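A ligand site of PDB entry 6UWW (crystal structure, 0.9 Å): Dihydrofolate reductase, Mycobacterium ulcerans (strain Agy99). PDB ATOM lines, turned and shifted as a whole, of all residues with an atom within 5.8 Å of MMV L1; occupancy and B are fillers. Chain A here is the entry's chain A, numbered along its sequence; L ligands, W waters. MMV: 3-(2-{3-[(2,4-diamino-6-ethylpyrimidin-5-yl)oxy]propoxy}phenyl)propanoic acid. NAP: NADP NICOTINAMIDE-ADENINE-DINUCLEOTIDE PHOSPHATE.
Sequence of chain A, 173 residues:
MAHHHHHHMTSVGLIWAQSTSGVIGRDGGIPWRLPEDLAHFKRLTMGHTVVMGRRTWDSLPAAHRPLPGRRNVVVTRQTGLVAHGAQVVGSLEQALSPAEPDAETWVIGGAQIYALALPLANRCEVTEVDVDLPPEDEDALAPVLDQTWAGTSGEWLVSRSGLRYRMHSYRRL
A ring nitrogen (ND1) of His 64 lies within hydrogen-bond range of an oxygen (O25) of MMV L1 (2.7 Å). A nitrogen (N4) of MMV L1 lies within hydrogen-bond range of the side-chain carboxylate of Asp 37, 2.7 Å away. An oxygen (O26) of MMV L1 is in salt-bridge range of the guanidinium group (NH1) of Arg 70. O of Ile 15 lies within hydrogen-bond range of N7 of MMV L1. The backbone carbonyl oxygen (O) of Ile 108 lies within hydrogen-bond range of a nitrogen (N7) of MMV L1 (3.0 Å). The side-chain hydroxyl (OH) of Tyr 114 lies within hydrogen-bond range of a nitrogen (N7) of MMV L1, 3.3 Å away. N of Ala 17 is in hydrogen-bond range of O7N of NAP L2 (2.9 Å). A nitrogen (N7N) of NAP L2 sits at hydrogen-bond distance from the backbone carbonyl oxygen (O) of Ala 17 (2.8 Å). N of Thr 56 sits at hydrogen-bond distance from O1A of NAP L2 (3.0 Å). The side-chain hydroxyl (OG1) of Thr 56 is in hydrogen-bond range of an oxygen (O1A) of NAP L2 (2.7 Å).
OG1 of Thr 127 is in hydrogen-bond range of OD1 of Asp 37, 2.7 Å away. The guanidinium group (NE) of Arg 70 sits at hydrogen-bond distance from the backbone carbonyl oxygen (O) of Pro 68. The side-chain hydroxyl of Thr 45 is in hydrogen-bond range of the guanidinium group of Arg 70 (3.1 Å). The side-chain hydroxyl (OH) of Tyr 114 sits at hydrogen-bond distance from the backbone carbonyl oxygen (O) of Ile 15. OG1 of Thr 45 lies within hydrogen-bond range of O of Phe 41, 2.8 Å away. The backbone NH of Gly 109 sits close to the side-chain hydroxyl of Tyr 114, 3.4 Å away. The backbone carbonyl oxygen of Trp 16 is in hydrogen-bond range of the backbone NH of Thr 127 (2.9 Å). The backbone NH (N) of Trp 16 is in hydrogen-bond range of the backbone carbonyl oxygen (O) of Glu 125, at 3.1 Å.
Residues that only touch MMV L1: Phe 41 (3.2 Å), Leu 67 (3.3 Å), Trp 16 (3.3 Å), Leu 38 (3.5 Å), Pro 61 (3.6 Å), Ile 30 (3.7 Å), Leu 60 (3.7 Å), Lys 42 (3.8 Å), Ala 17 (3.8 Å) and Thr 127 (3.9 Å). Within 4 Å of MMV L1: Ile 15, Trp 16, Ala 17, Ile 30, Asp 37, Leu 38, Phe 41, Lys 42, Leu 60, Pro 61, His 64, Leu 67, Arg 70, Ile 108, Tyr 114 and Thr 127. The nearest printed residue that does not touch MMV L1 is Pro 68 (4.002 Å).
Water W1 lies within hydrogen-bond range of OG1 of Thr 127 (2.9 Å), O of Glu 125 (3.0 Å), N8 of MMV L1 (3.0 Å), NE2 of His 40 (3.0 Å) and O of Trp 16 (3.2 Å).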
ATOM      1  N   ILE A  15      -4.207 -30.832  -9.150  1.00  0.00           N
ATOM      2  CA  ILE A  15      -2.787 -30.856  -8.851  1.00  0.00           C
ATOM      3  C   ILE A  15      -2.174 -29.620  -9.488  1.00  0.00           C
ATOM      4  O   ILE A  15      -2.431 -29.362 -10.665  1.00  0.00           O
ATOM      5  CB  ILE A  15      -2.119 -32.190  -9.312  1.00  0.00           C
ATOM      6  CG1 ILE A  15      -0.637 -32.233  -8.949  1.00  0.00           C
ATOM      7  CG2 ILE A  15      -2.356 -32.488 -10.783  1.00  0.00           C
ATOM      8  CD1 ILE A  15      -0.045 -33.607  -9.005  1.00  0.00           C
ATOM      9  N   TRP A  16      -1.406 -28.856  -8.722  1.00  0.00           N
ATOM     10  CA  TRP A  16      -0.754 -27.659  -9.232  1.00  0.00           C
ATOM     11  C   TRP A  16       0.504 -27.369  -8.427  1.00  0.00           C
ATOM     12  O   TRP A  16       0.647 -27.828  -7.299  1.00  0.00           O
ATOM     13  CB  TRP A  16      -1.666 -26.420  -9.250  1.00  0.00           C
ATOM     14  CG  TRP A  16      -1.981 -25.756  -7.935  1.00  0.00           C
ATOM     15  CD1 TRP A  16      -1.267 -24.776  -7.327  1.00  0.00           C
ATOM     16  CD2 TRP A  16      -3.141 -25.972  -7.113  1.00  0.00           C
ATOM     17  NE1 TRP A  16      -1.908 -24.352  -6.182  1.00  0.00           N
ATOM     18  CE2 TRP A  16      -3.064 -25.069  -6.027  1.00  0.00           C
ATOM     19  CE3 TRP A  16      -4.246 -26.828  -7.201  1.00  0.00           C
ATOM     20  CZ2 TRP A  16      -4.038 -25.015  -5.039  1.00  0.00           C
ATOM     21  CZ3 TRP A  16      -5.212 -26.769  -6.216  1.00  0.00           C
ATOM     22  CH2 TRP A  16      -5.105 -25.870  -5.152  1.00  0.00           C
ATOM     23  N   ALA A  17       1.368 -26.551  -9.028  1.00  0.00           N
ATOM     24  CA  ALA A  17       2.529 -25.979  -8.370  1.00  0.00           C
ATOM     25  C   ALA A  17       2.420 -24.457  -8.421  1.00  0.00           C
ATOM     26  O   ALA A  17       2.137 -23.887  -9.474  1.00  0.00           O
ATOM     27  CB  ALA A  17       3.826 -26.443  -9.050  1.00  0.00           C
ATOM     28  N   ILE A  30       5.644 -21.947 -17.135  1.00  0.00           N
ATOM     29  CA  ILE A  30       5.758 -21.970 -15.689  1.00  0.00           C
ATOM     30  C   ILE A  30       7.062 -21.268 -15.331  1.00  0.00           C
ATOM     31  O   ILE A  30       8.123 -21.672 -15.820  1.00  0.00           O
ATOM     32  CB  ILE A  30       5.721 -23.407 -15.142  1.00  0.00           C
ATOM     33  CG1 ILE A  30       4.371 -24.056 -15.477  1.00  0.00           C
ATOM     34  CG2 ILE A  30       5.987 -23.412 -13.657  1.00  0.00           C
ATOM     35  CD1 ILE A  30       4.282 -25.509 -15.134  1.00  0.00           C
ATOM     36  N   ASP A  37       9.326 -31.256  -8.563  1.00  0.00           N
ATOM     37  CA  ASP A  37       7.892 -31.125  -8.780  1.00  0.00           C
ATOM     38  C   ASP A  37       7.458 -31.866 -10.035  1.00  0.00           C
ATOM     39  O   ASP A  37       6.394 -32.494 -10.039  1.00  0.00           O
ATOM     40  CB  ASP A  37       7.495 -29.655  -8.890  1.00  0.00           C
ATOM     41  CG  ASP A  37       6.041 -29.536  -9.290  1.00  0.00           C
ATOM     42  OD1 ASP A  37       5.185 -29.891  -8.452  1.00  0.00           O
ATOM     43  OD2 ASP A  37       5.765 -29.153 -10.460  1.00  0.00           O
ATOM     44  N   LEU A  38       8.247 -31.803 -11.103  1.00  0.00           N
ATOM     45  CA  LEU A  38       7.908 -32.593 -12.282  1.00  0.00           C
ATOM     46  C   LEU A  38       7.862 -34.068 -11.954  1.00  0.00           C
ATOM     47  O   LEU A  38       6.961 -34.790 -12.396  1.00  0.00           O
ATOM     48  CB  LEU A  38       8.890 -32.279 -13.399  1.00  0.00           C
ATOM     49  CG  LEU A  38       8.705 -33.130 -14.642  1.00  0.00           C
ATOM     50  CD1 LEU A  38       7.276 -33.066 -15.144  1.00  0.00           C
ATOM     51  CD2 LEU A  38       9.682 -32.687 -15.714  1.00  0.00           C
ATOM     52  N   HIS A  40       7.226 -35.450  -8.986  1.00  0.00           N
ATOM     53  CA  HIS A  40       6.005 -35.626  -8.198  1.00  0.00           C
ATOM     54  C   HIS A  40       4.771 -35.678  -9.094  1.00  0.00           C
ATOM     55  O   HIS A  40       3.907 -36.538  -8.930  1.00  0.00           O
ATOM     56  CB  HIS A  40       5.979 -34.434  -7.236  1.00  0.00           C
ATOM     57  CG  HIS A  40       4.706 -34.224  -6.492  1.00  0.00           C
ATOM     58  ND1 HIS A  40       4.309 -34.979  -5.418  1.00  0.00           N
ATOM     59  CD2 HIS A  40       3.788 -33.236  -6.627  1.00  0.00           C
ATOM     60  CE1 HIS A  40       3.185 -34.483  -4.923  1.00  0.00           C
ATOM     61  NE2 HIS A  40       2.850 -33.423  -5.644  1.00  0.00           N
ATOM     62  N   PHE A  41       4.673 -34.752 -10.042  1.00  0.00           N
ATOM     63  CA  PHE A  41       3.545 -34.702 -10.954  1.00  0.00           C
ATOM     64  C   PHE A  41       3.439 -35.989 -11.774  1.00  0.00           C
ATOM     65  O   PHE A  41       2.357 -36.555 -11.915  1.00  0.00           O
ATOM     66  CB  PHE A  41       3.705 -33.476 -11.872  1.00  0.00           C
ATOM     67  CG  PHE A  41       2.646 -33.375 -12.931  1.00  0.00           C
ATOM     68  CD1 PHE A  41       1.361 -32.942 -12.617  1.00  0.00           C
ATOM     69  CD2 PHE A  41       2.922 -33.731 -14.245  1.00  0.00           C
ATOM     70  CE1 PHE A  41       0.367 -32.886 -13.579  1.00  0.00           C
ATOM     71  CE2 PHE A  41       1.937 -33.679 -15.221  1.00  0.00           C
ATOM     72  CZ  PHE A  41       0.654 -33.249 -14.876  1.00  0.00           C
ATOM     73  N   LYS A  42       4.564 -36.456 -12.314  1.00  0.00           N
ATOM     74  CA  LYS A  42       4.593 -37.715 -13.068  1.00  0.00           C
ATOM     75  C   LYS A  42       4.175 -38.887 -12.198  1.00  0.00           C
ATOM     76  O   LYS A  42       3.407 -39.755 -12.635  1.00  0.00           O
ATOM     77  CB  LYS A  42       6.012 -37.991 -13.551  1.00  0.00           C
ATOM     78  CG  LYS A  42       6.452 -37.201 -14.740  1.00  0.00           C
ATOM     79  CD  LYS A  42       7.904 -37.537 -15.049  1.00  0.00           C
ATOM     80  CE  LYS A  42       8.383 -36.770 -16.262  1.00  0.00           C
ATOM     81  NZ  LYS A  42       9.850 -37.017 -16.476  1.00  0.00           N
ATOM     82  N   THR A  45       0.317 -38.751 -11.516  1.00  0.00           N
ATOM     83  CA  THR A  45      -0.602 -38.786 -12.627  1.00  0.00           C
ATOM     84  C   THR A  45      -0.430 -39.996 -13.556  1.00  0.00           C
ATOM     85  O   THR A  45      -1.368 -40.308 -14.295  1.00  0.00           O
ATOM     86  CB  THR A  45      -0.565 -37.497 -13.461  1.00  0.00           C
ATOM     87  OG1 THR A  45       0.728 -37.296 -14.043  1.00  0.00           O
ATOM     88  CG2 THR A  45      -1.002 -36.265 -12.639  1.00  0.00           C
ATOM     89  N   THR A  56      -3.351 -24.664 -21.388  1.00  0.00           N
ATOM     90  CA  THR A  56      -2.367 -25.566 -20.803  1.00  0.00           C
ATOM     91  C   THR A  56      -1.914 -26.609 -21.828  1.00  0.00           C
ATOM     92  O   THR A  56      -0.711 -26.918 -21.907  1.00  0.00           O
ATOM     93  CB  THR A  56      -2.926 -26.189 -19.529  1.00  0.00           C
ATOM     94  OG1 THR A  56      -3.029 -25.178 -18.524  1.00  0.00           O
ATOM     95  CG2 THR A  56      -2.014 -27.272 -18.978  1.00  0.00           C
ATOM     96  N   SER A  59       0.652 -25.061 -23.835  1.00  0.00           N
ATOM     97  CA  SER A  59       1.860 -24.781 -23.076  1.00  0.00           C
ATOM     98  C   SER A  59       2.770 -25.992 -22.910  1.00  0.00           C
ATOM     99  O   SER A  59       3.908 -25.828 -22.447  1.00  0.00           O
ATOM    100  CB  SER A  59       1.493 -24.244 -21.678  1.00  0.00           C
ATOM    101  OG  SER A  59       1.123 -25.282 -20.773  1.00  0.00           O
ATOM    102  N   LEU A  60       2.301 -27.194 -23.227  1.00  0.00           N
ATOM    103  CA  LEU A  60       3.091 -28.379 -22.933  1.00  0.00           C
ATOM    104  C   LEU A  60       4.317 -28.416 -23.823  1.00  0.00           C
ATOM    105  O   LEU A  60       4.211 -28.190 -25.032  1.00  0.00           O
ATOM    106  CB  LEU A  60       2.272 -29.649 -23.158  1.00  0.00           C
ATOM    107  CG  LEU A  60       1.123 -29.864 -22.190  1.00  0.00           C
ATOM    108  CD1 LEU A  60       0.297 -31.057 -22.622  1.00  0.00           C
ATOM    109  CD2 LEU A  60       1.629 -30.052 -20.790  1.00  0.00           C
ATOM    110  N   PRO A  61       5.493 -28.740 -23.281  1.00  0.00           N
ATOM    111  CA  PRO A  61       6.679 -28.870 -24.128  1.00  0.00           C
ATOM    112  C   PRO A  61       6.521 -30.017 -25.121  1.00  0.00           C
ATOM    113  O   PRO A  61       5.765 -30.964 -24.903  1.00  0.00           O
ATOM    114  CB  PRO A  61       7.809 -29.165 -23.133  1.00  0.00           C
ATOM    115  CG  PRO A  61       7.282 -28.908 -21.792  1.00  0.00           C
ATOM    116  CD  PRO A  61       5.788 -28.939 -21.845  1.00  0.00           C
ATOM    117  N   HIS A  64       6.175 -33.698 -24.450  1.00  0.00           N
ATOM    118  CA  HIS A  64       5.160 -33.950 -23.444  1.00  0.00           C
ATOM    119  C   HIS A  64       3.784 -33.533 -23.929  1.00  0.00           C
ATOM    120  O   HIS A  64       2.895 -33.350 -23.090  1.00  0.00           O
ATOM    121  CB  HIS A  64       5.524 -33.214 -22.162  1.00  0.00           C
ATOM    122  CG  HIS A  64       6.869 -33.607 -21.634  1.00  0.00           C
ATOM    123  ND1 HIS A  64       7.048 -34.602 -20.701  1.00  0.00           N
ATOM    124  CD2 HIS A  64       8.107 -33.178 -21.979  1.00  0.00           C
ATOM    125  CE1 HIS A  64       8.342 -34.752 -20.463  1.00  0.00           C
ATOM    126  NE2 HIS A  64       9.001 -33.898 -21.215  1.00  0.00           N
ATOM    127  N   LEU A  67       0.900 -35.740 -22.874  1.00  0.00           N
ATOM    128  CA  LEU A  67       1.611 -36.248 -21.707  1.00  0.00           C
ATOM    129  C   LEU A  67       1.660 -37.773 -21.805  1.00  0.00           C
ATOM    130  O   LEU A  67       0.603 -38.417 -21.842  1.00  0.00           O
ATOM    131  CB  LEU A  67       0.900 -35.806 -20.441  1.00  0.00           C
ATOM    132  CG  LEU A  67       0.986 -34.297 -20.188  1.00  0.00           C
ATOM    133  CD1 LEU A  67      -0.095 -33.841 -19.236  1.00  0.00           C
ATOM    134  CD2 LEU A  67       2.337 -33.915 -19.682  1.00  0.00           C
ATOM    135  N   PRO A  68       2.840 -38.388 -21.883  1.00  0.00           N
ATOM    136  CA  PRO A  68       2.904 -39.829 -22.154  1.00  0.00           C
ATOM    137  C   PRO A  68       2.344 -40.643 -20.993  1.00  0.00           C
ATOM    138  O   PRO A  68       2.520 -40.309 -19.824  1.00  0.00           O
ATOM    139  CB  PRO A  68       4.403 -40.096 -22.347  1.00  0.00           C
ATOM    140  CG  PRO A  68       5.090 -38.936 -21.647  1.00  0.00           C
ATOM    141  CD  PRO A  68       4.182 -37.768 -21.928  1.00  0.00           C
ATOM    142  N   ARG A  70      -0.719 -41.271 -20.021  1.00  0.00           N
ATOM    143  CA  ARG A  70      -1.902 -40.732 -19.379  1.00  0.00           C
ATOM    144  C   ARG A  70      -2.933 -40.455 -20.452  1.00  0.00           C
ATOM    145  O   ARG A  70      -2.591 -40.174 -21.597  1.00  0.00           O
ATOM    146  CB  ARG A  70      -1.521 -39.440 -18.651  1.00  0.00           C
ATOM    147  CG  ARG A  70      -0.764 -39.756 -17.377  1.00  0.00           C
ATOM    148  CD  ARG A  70       0.184 -38.672 -16.917  1.00  0.00           C
ATOM    149  NE  ARG A  70       1.390 -38.634 -17.753  1.00  0.00           N
ATOM    150  CZ  ARG A  70       2.375 -37.770 -17.589  1.00  0.00           C
ATOM    151  NH1 ARG A  70       2.337 -36.857 -16.622  1.00  0.00           N
ATOM    152  NH2 ARG A  70       3.411 -37.788 -18.410  1.00  0.00           N
ATOM    153  N   VAL A 107      -7.213 -32.957 -12.559  1.00  0.00           N
ATOM    154  CA  VAL A 107      -7.278 -31.681 -13.247  1.00  0.00           C
ATOM    155  C   VAL A 107      -5.942 -30.989 -13.061  1.00  0.00           C
ATOM    156  O   VAL A 107      -5.527 -30.719 -11.932  1.00  0.00           O
ATOM    157  CB  VAL A 107      -8.445 -30.839 -12.711  1.00  0.00           C
ATOM    158  CG1 VAL A 107      -8.427 -29.458 -13.353  1.00  0.00           C
ATOM    159  CG2 VAL A 107      -9.780 -31.558 -12.960  1.00  0.00           C
ATOM    160  N   ILE A 108      -5.255 -30.759 -14.179  1.00  0.00           N
ATOM    161  CA  ILE A 108      -3.860 -30.364 -14.193  1.00  0.00           C
ATOM    162  C   ILE A 108      -3.653 -28.918 -14.643  1.00  0.00           C
ATOM    163  O   ILE A 108      -2.507 -28.516 -14.866  1.00  0.00           O
ATOM    164  CB  ILE A 108      -3.001 -31.332 -15.022  1.00  0.00           C
ATOM    165  CG1 ILE A 108      -3.301 -31.221 -16.503  1.00  0.00           C
ATOM    166  CG2 ILE A 108      -3.160 -32.750 -14.507  1.00  0.00           C
ATOM    167  CD1 ILE A 108      -2.186 -31.801 -17.394  1.00  0.00           C
ATOM    168  N   GLY A 109      -4.727 -28.149 -14.746  1.00  0.00           N
ATOM    169  CA  GLY A 109      -4.660 -26.721 -14.971  1.00  0.00           C
ATOM    170  C   GLY A 109      -5.351 -26.313 -16.256  1.00  0.00           C
ATOM    171  O   GLY A 109      -5.903 -27.141 -16.969  1.00  0.00           O
ATOM    172  N   TYR A 114      -8.978 -24.639 -13.173  1.00  0.00           N
ATOM    173  CA  TYR A 114      -8.986 -24.915 -11.747  1.00  0.00           C
ATOM    174  C   TYR A 114     -10.193 -24.268 -11.073  1.00  0.00           C
ATOM    175  O   TYR A 114     -10.778 -24.842 -10.147  1.00  0.00           O
ATOM    176  CB  TYR A 114      -7.719 -24.417 -11.049  1.00  0.00           C
ATOM    177  CG  TYR A 114      -6.445 -25.175 -11.332  1.00  0.00           C
ATOM    178  CD1 TYR A 114      -6.399 -26.557 -11.301  1.00  0.00           C
ATOM    179  CD2 TYR A 114      -5.266 -24.481 -11.579  1.00  0.00           C
ATOM    180  CE1 TYR A 114      -5.206 -27.226 -11.540  1.00  0.00           C
ATOM    181  CE2 TYR A 114      -4.079 -25.132 -11.806  1.00  0.00           C
ATOM    182  CZ  TYR A 114      -4.048 -26.508 -11.803  1.00  0.00           C
ATOM    183  OH  TYR A 114      -2.862 -27.118 -12.098  1.00  0.00           O
ATOM    184  N   GLU A 125      -3.511 -31.634  -4.605  1.00  0.00           N
ATOM    185  CA  GLU A 125      -2.099 -31.894  -4.348  1.00  0.00           C
ATOM    186  C   GLU A 125      -1.326 -30.672  -4.829  1.00  0.00           C
ATOM    187  O   GLU A 125      -1.304 -30.391  -6.037  1.00  0.00           O
ATOM    188  CB  GLU A 125      -1.659 -33.172  -5.050  1.00  0.00           C
ATOM    189  CG  GLU A 125      -2.311 -34.429  -4.504  1.00  0.00           C
ATOM    190  CD  GLU A 125      -1.942 -34.728  -3.055  1.00  0.00           C
ATOM    191  OE1 GLU A 125      -0.855 -34.330  -2.602  1.00  0.00           O
ATOM    192  OE2 GLU A 125      -2.754 -35.395  -2.358  1.00  0.00           O
ATOM    193  N   THR A 127       2.101 -28.157  -4.806  1.00  0.00           N
ATOM    194  CA  THR A 127       3.509 -27.878  -4.538  1.00  0.00           C
ATOM    195  C   THR A 127       3.664 -26.383  -4.342  1.00  0.00           C
ATOM    196  O   THR A 127       3.218 -25.604  -5.180  1.00  0.00           O
ATOM    197  CB  THR A 127       4.394 -28.332  -5.696  1.00  0.00           C
ATOM    198  OG1 THR A 127       4.158 -29.717  -5.935  1.00  0.00           O
ATOM    199  CG2 THR A 127       5.861 -28.084  -5.383  1.00  0.00           C
HETATM  200  C1  MMV L   1       0.798 -29.422 -12.404  1.00  0.00           C
HETATM  201  N2  MMV L   1       1.009 -29.758 -11.150  1.00  0.00           N
HETATM  202  C3  MMV L   1       2.280 -29.778 -10.764  1.00  0.00           C
HETATM  203  N4  MMV L   1       3.295 -29.469 -11.572  1.00  0.00           N
HETATM  204  C5  MMV L   1       3.096 -29.157 -12.860  1.00  0.00           C
HETATM  205  C6  MMV L   1       1.810 -29.125 -13.327  1.00  0.00           C
HETATM  206  N7  MMV L   1      -0.549 -29.394 -12.815  1.00  0.00           N
HETATM  207  N8  MMV L   1       2.564 -30.129  -9.440  1.00  0.00           N
HETATM  208  C9  MMV L   1       4.311 -28.877 -13.697  1.00  0.00           C
HETATM  209  C10 MMV L   1       5.092 -30.175 -13.957  1.00  0.00           C
HETATM  210  O11 MMV L   1       1.511 -28.774 -14.624  1.00  0.00           O
HETATM  211  C12 MMV L   1       1.241 -29.866 -15.516  1.00  0.00           C
HETATM  212  C13 MMV L   1       1.152 -29.292 -16.920  1.00  0.00           C
HETATM  213  C14 MMV L   1       2.498 -28.781 -17.396  1.00  0.00           C
HETATM  214  O15 MMV L   1       3.358 -29.899 -17.486  1.00  0.00           O
HETATM  215  C16 MMV L   1       4.680 -29.707 -17.746  1.00  0.00           C
HETATM  216  C17 MMV L   1       5.491 -30.823 -17.775  1.00  0.00           C
HETATM  217  C18 MMV L   1       6.858 -30.655 -18.018  1.00  0.00           C
HETATM  218  C19 MMV L   1       7.378 -29.378 -18.239  1.00  0.00           C
HETATM  219  C20 MMV L   1       6.543 -28.273 -18.221  1.00  0.00           C
HETATM  220  C21 MMV L   1       5.192 -28.422 -17.975  1.00  0.00           C
HETATM  221  C22 MMV L   1       4.871 -32.191 -17.510  1.00  0.00           C
HETATM  222  C23 MMV L   1       5.518 -33.306 -18.312  1.00  0.00           C
HETATM  223  C24 MMV L   1       5.053 -34.706 -17.952  1.00  0.00           C
HETATM  224  O25 MMV L   1       5.368 -35.569 -18.802  1.00  0.00           O
HETATM  225  O26 MMV L   1       4.375 -34.945 -16.911  1.00  0.00           O
HETATM  226  PA  NAP L   2      -6.305 -22.815 -19.093  1.00  0.00           P
HETATM  227  O1A NAP L   2      -5.274 -23.881 -19.261  1.00  0.00           O
HETATM  228  O2A NAP L   2      -7.184 -22.857 -17.919  1.00  0.00           O
HETATM  229  O5B NAP L   2      -7.100 -22.845 -20.486  1.00  0.00           O
HETATM  230  C5B NAP L   2      -8.127 -21.900 -20.737  1.00  0.00           C
HETATM  231  C4B NAP L   2      -8.938 -22.389 -21.937  1.00  0.00           C
HETATM  232  O4B NAP L   2      -9.744 -23.393 -21.536  1.00  0.00           O
HETATM  233  C3B NAP L   2      -9.825 -21.296 -22.563  1.00  0.00           C
HETATM  234  O3B NAP L   2      -9.117 -20.389 -23.358  1.00  0.00           O
HETATM  235  C2B NAP L   2     -10.839 -22.254 -23.243  1.00  0.00           C
HETATM  236  O2B NAP L   2     -10.220 -22.804 -24.466  1.00  0.00           O
HETATM  237  C1B NAP L   2     -11.016 -23.293 -22.345  1.00  0.00           C
HETATM  238  N9A NAP L   2     -12.116 -23.108 -21.396  1.00  0.00           N
HETATM  239  C8A NAP L   2     -12.194 -22.344 -20.284  1.00  0.00           C
HETATM  240  N7A NAP L   2     -13.424 -22.415 -19.758  1.00  0.00           N
HETATM  241  C5A NAP L   2     -14.124 -23.242 -20.565  1.00  0.00           C
HETATM  242  C6A NAP L   2     -15.441 -23.690 -20.522  1.00  0.00           C
HETATM  243  N6A NAP L   2     -16.421 -23.357 -19.522  1.00  0.00           N
HETATM  244  N1A NAP L   2     -15.872 -24.509 -21.462  1.00  0.00           N
HETATM  245  C2A NAP L   2     -15.028 -24.911 -22.470  1.00  0.00           C
HETATM  246  N3A NAP L   2     -13.763 -24.509 -22.554  1.00  0.00           N
HETATM  247  C4A NAP L   2     -13.344 -23.665 -21.580  1.00  0.00           C
HETATM  248  O3  NAP L   2      -5.605 -21.373 -19.244  1.00  0.00           O
HETATM  249  PN  NAP L   2      -4.814 -20.411 -18.214  1.00  0.00           P
HETATM  250  O1N NAP L   2      -5.638 -20.099 -17.014  1.00  0.00           O
HETATM  251  O2N NAP L   2      -4.336 -19.257 -19.051  1.00  0.00           O
HETATM  252  O5D NAP L   2      -3.576 -21.321 -17.702  1.00  0.00           O
HETATM  253  C5D NAP L   2      -2.443 -21.548 -18.542  1.00  0.00           C
HETATM  254  C4D NAP L   2      -1.203 -21.095 -17.766  1.00  0.00           C
HETATM  255  O4D NAP L   2      -1.084 -21.808 -16.597  1.00  0.00           O
HETATM  256  C3D NAP L   2       0.120 -21.273 -18.553  1.00  0.00           C
HETATM  257  O3D NAP L   2       1.038 -20.286 -18.181  1.00  0.00           O
HETATM  258  C2D NAP L   2       0.557 -22.639 -17.973  1.00  0.00           C
HETATM  259  O2D NAP L   2       1.995 -22.786 -18.206  1.00  0.00           O
HETATM  260  C1D NAP L   2       0.272 -22.561 -16.644  1.00  0.00           C
HETATM  261  N1N NAP L   2       0.047 -23.781 -15.874  1.00  0.00           N
HETATM  262  C2N NAP L   2       0.683 -23.936 -14.675  1.00  0.00           C
HETATM  263  C3N NAP L   2       0.486 -25.074 -13.900  1.00  0.00           C
HETATM  264  C7N NAP L   2       1.160 -25.234 -12.586  1.00  0.00           C
HETATM  265  O7N NAP L   2       0.855 -26.131 -11.834  1.00  0.00           O
HETATM  266  N7N NAP L   2       2.161 -24.335 -12.249  1.00  0.00           N
HETATM  267  C4N NAP L   2      -0.395 -26.033 -14.352  1.00  0.00           C
HETATM  268  C5N NAP L   2      -1.018 -25.882 -15.556  1.00  0.00           C
HETATM  269  C6N NAP L   2      -0.805 -24.748 -16.325  1.00  0.00           C
HETATM  270  P2B NAP L   2     -10.478 -22.143 -25.921  1.00  0.00           P
HETATM  271  O1X NAP L   2     -11.970 -22.099 -26.131  1.00  0.00           O
HETATM  272  O2X NAP L   2      -9.841 -20.754 -25.884  1.00  0.00           O
HETATM  273  O3X NAP L   2      -9.752 -23.101 -26.851  1.00  0.00           O
HETATM  274  O   HOH W   1       1.601 -30.865  -6.681  1.00  0.00           O
HETATM  275  O   HOH W   2       6.986 -37.944 -19.007  1.00  0.00           O
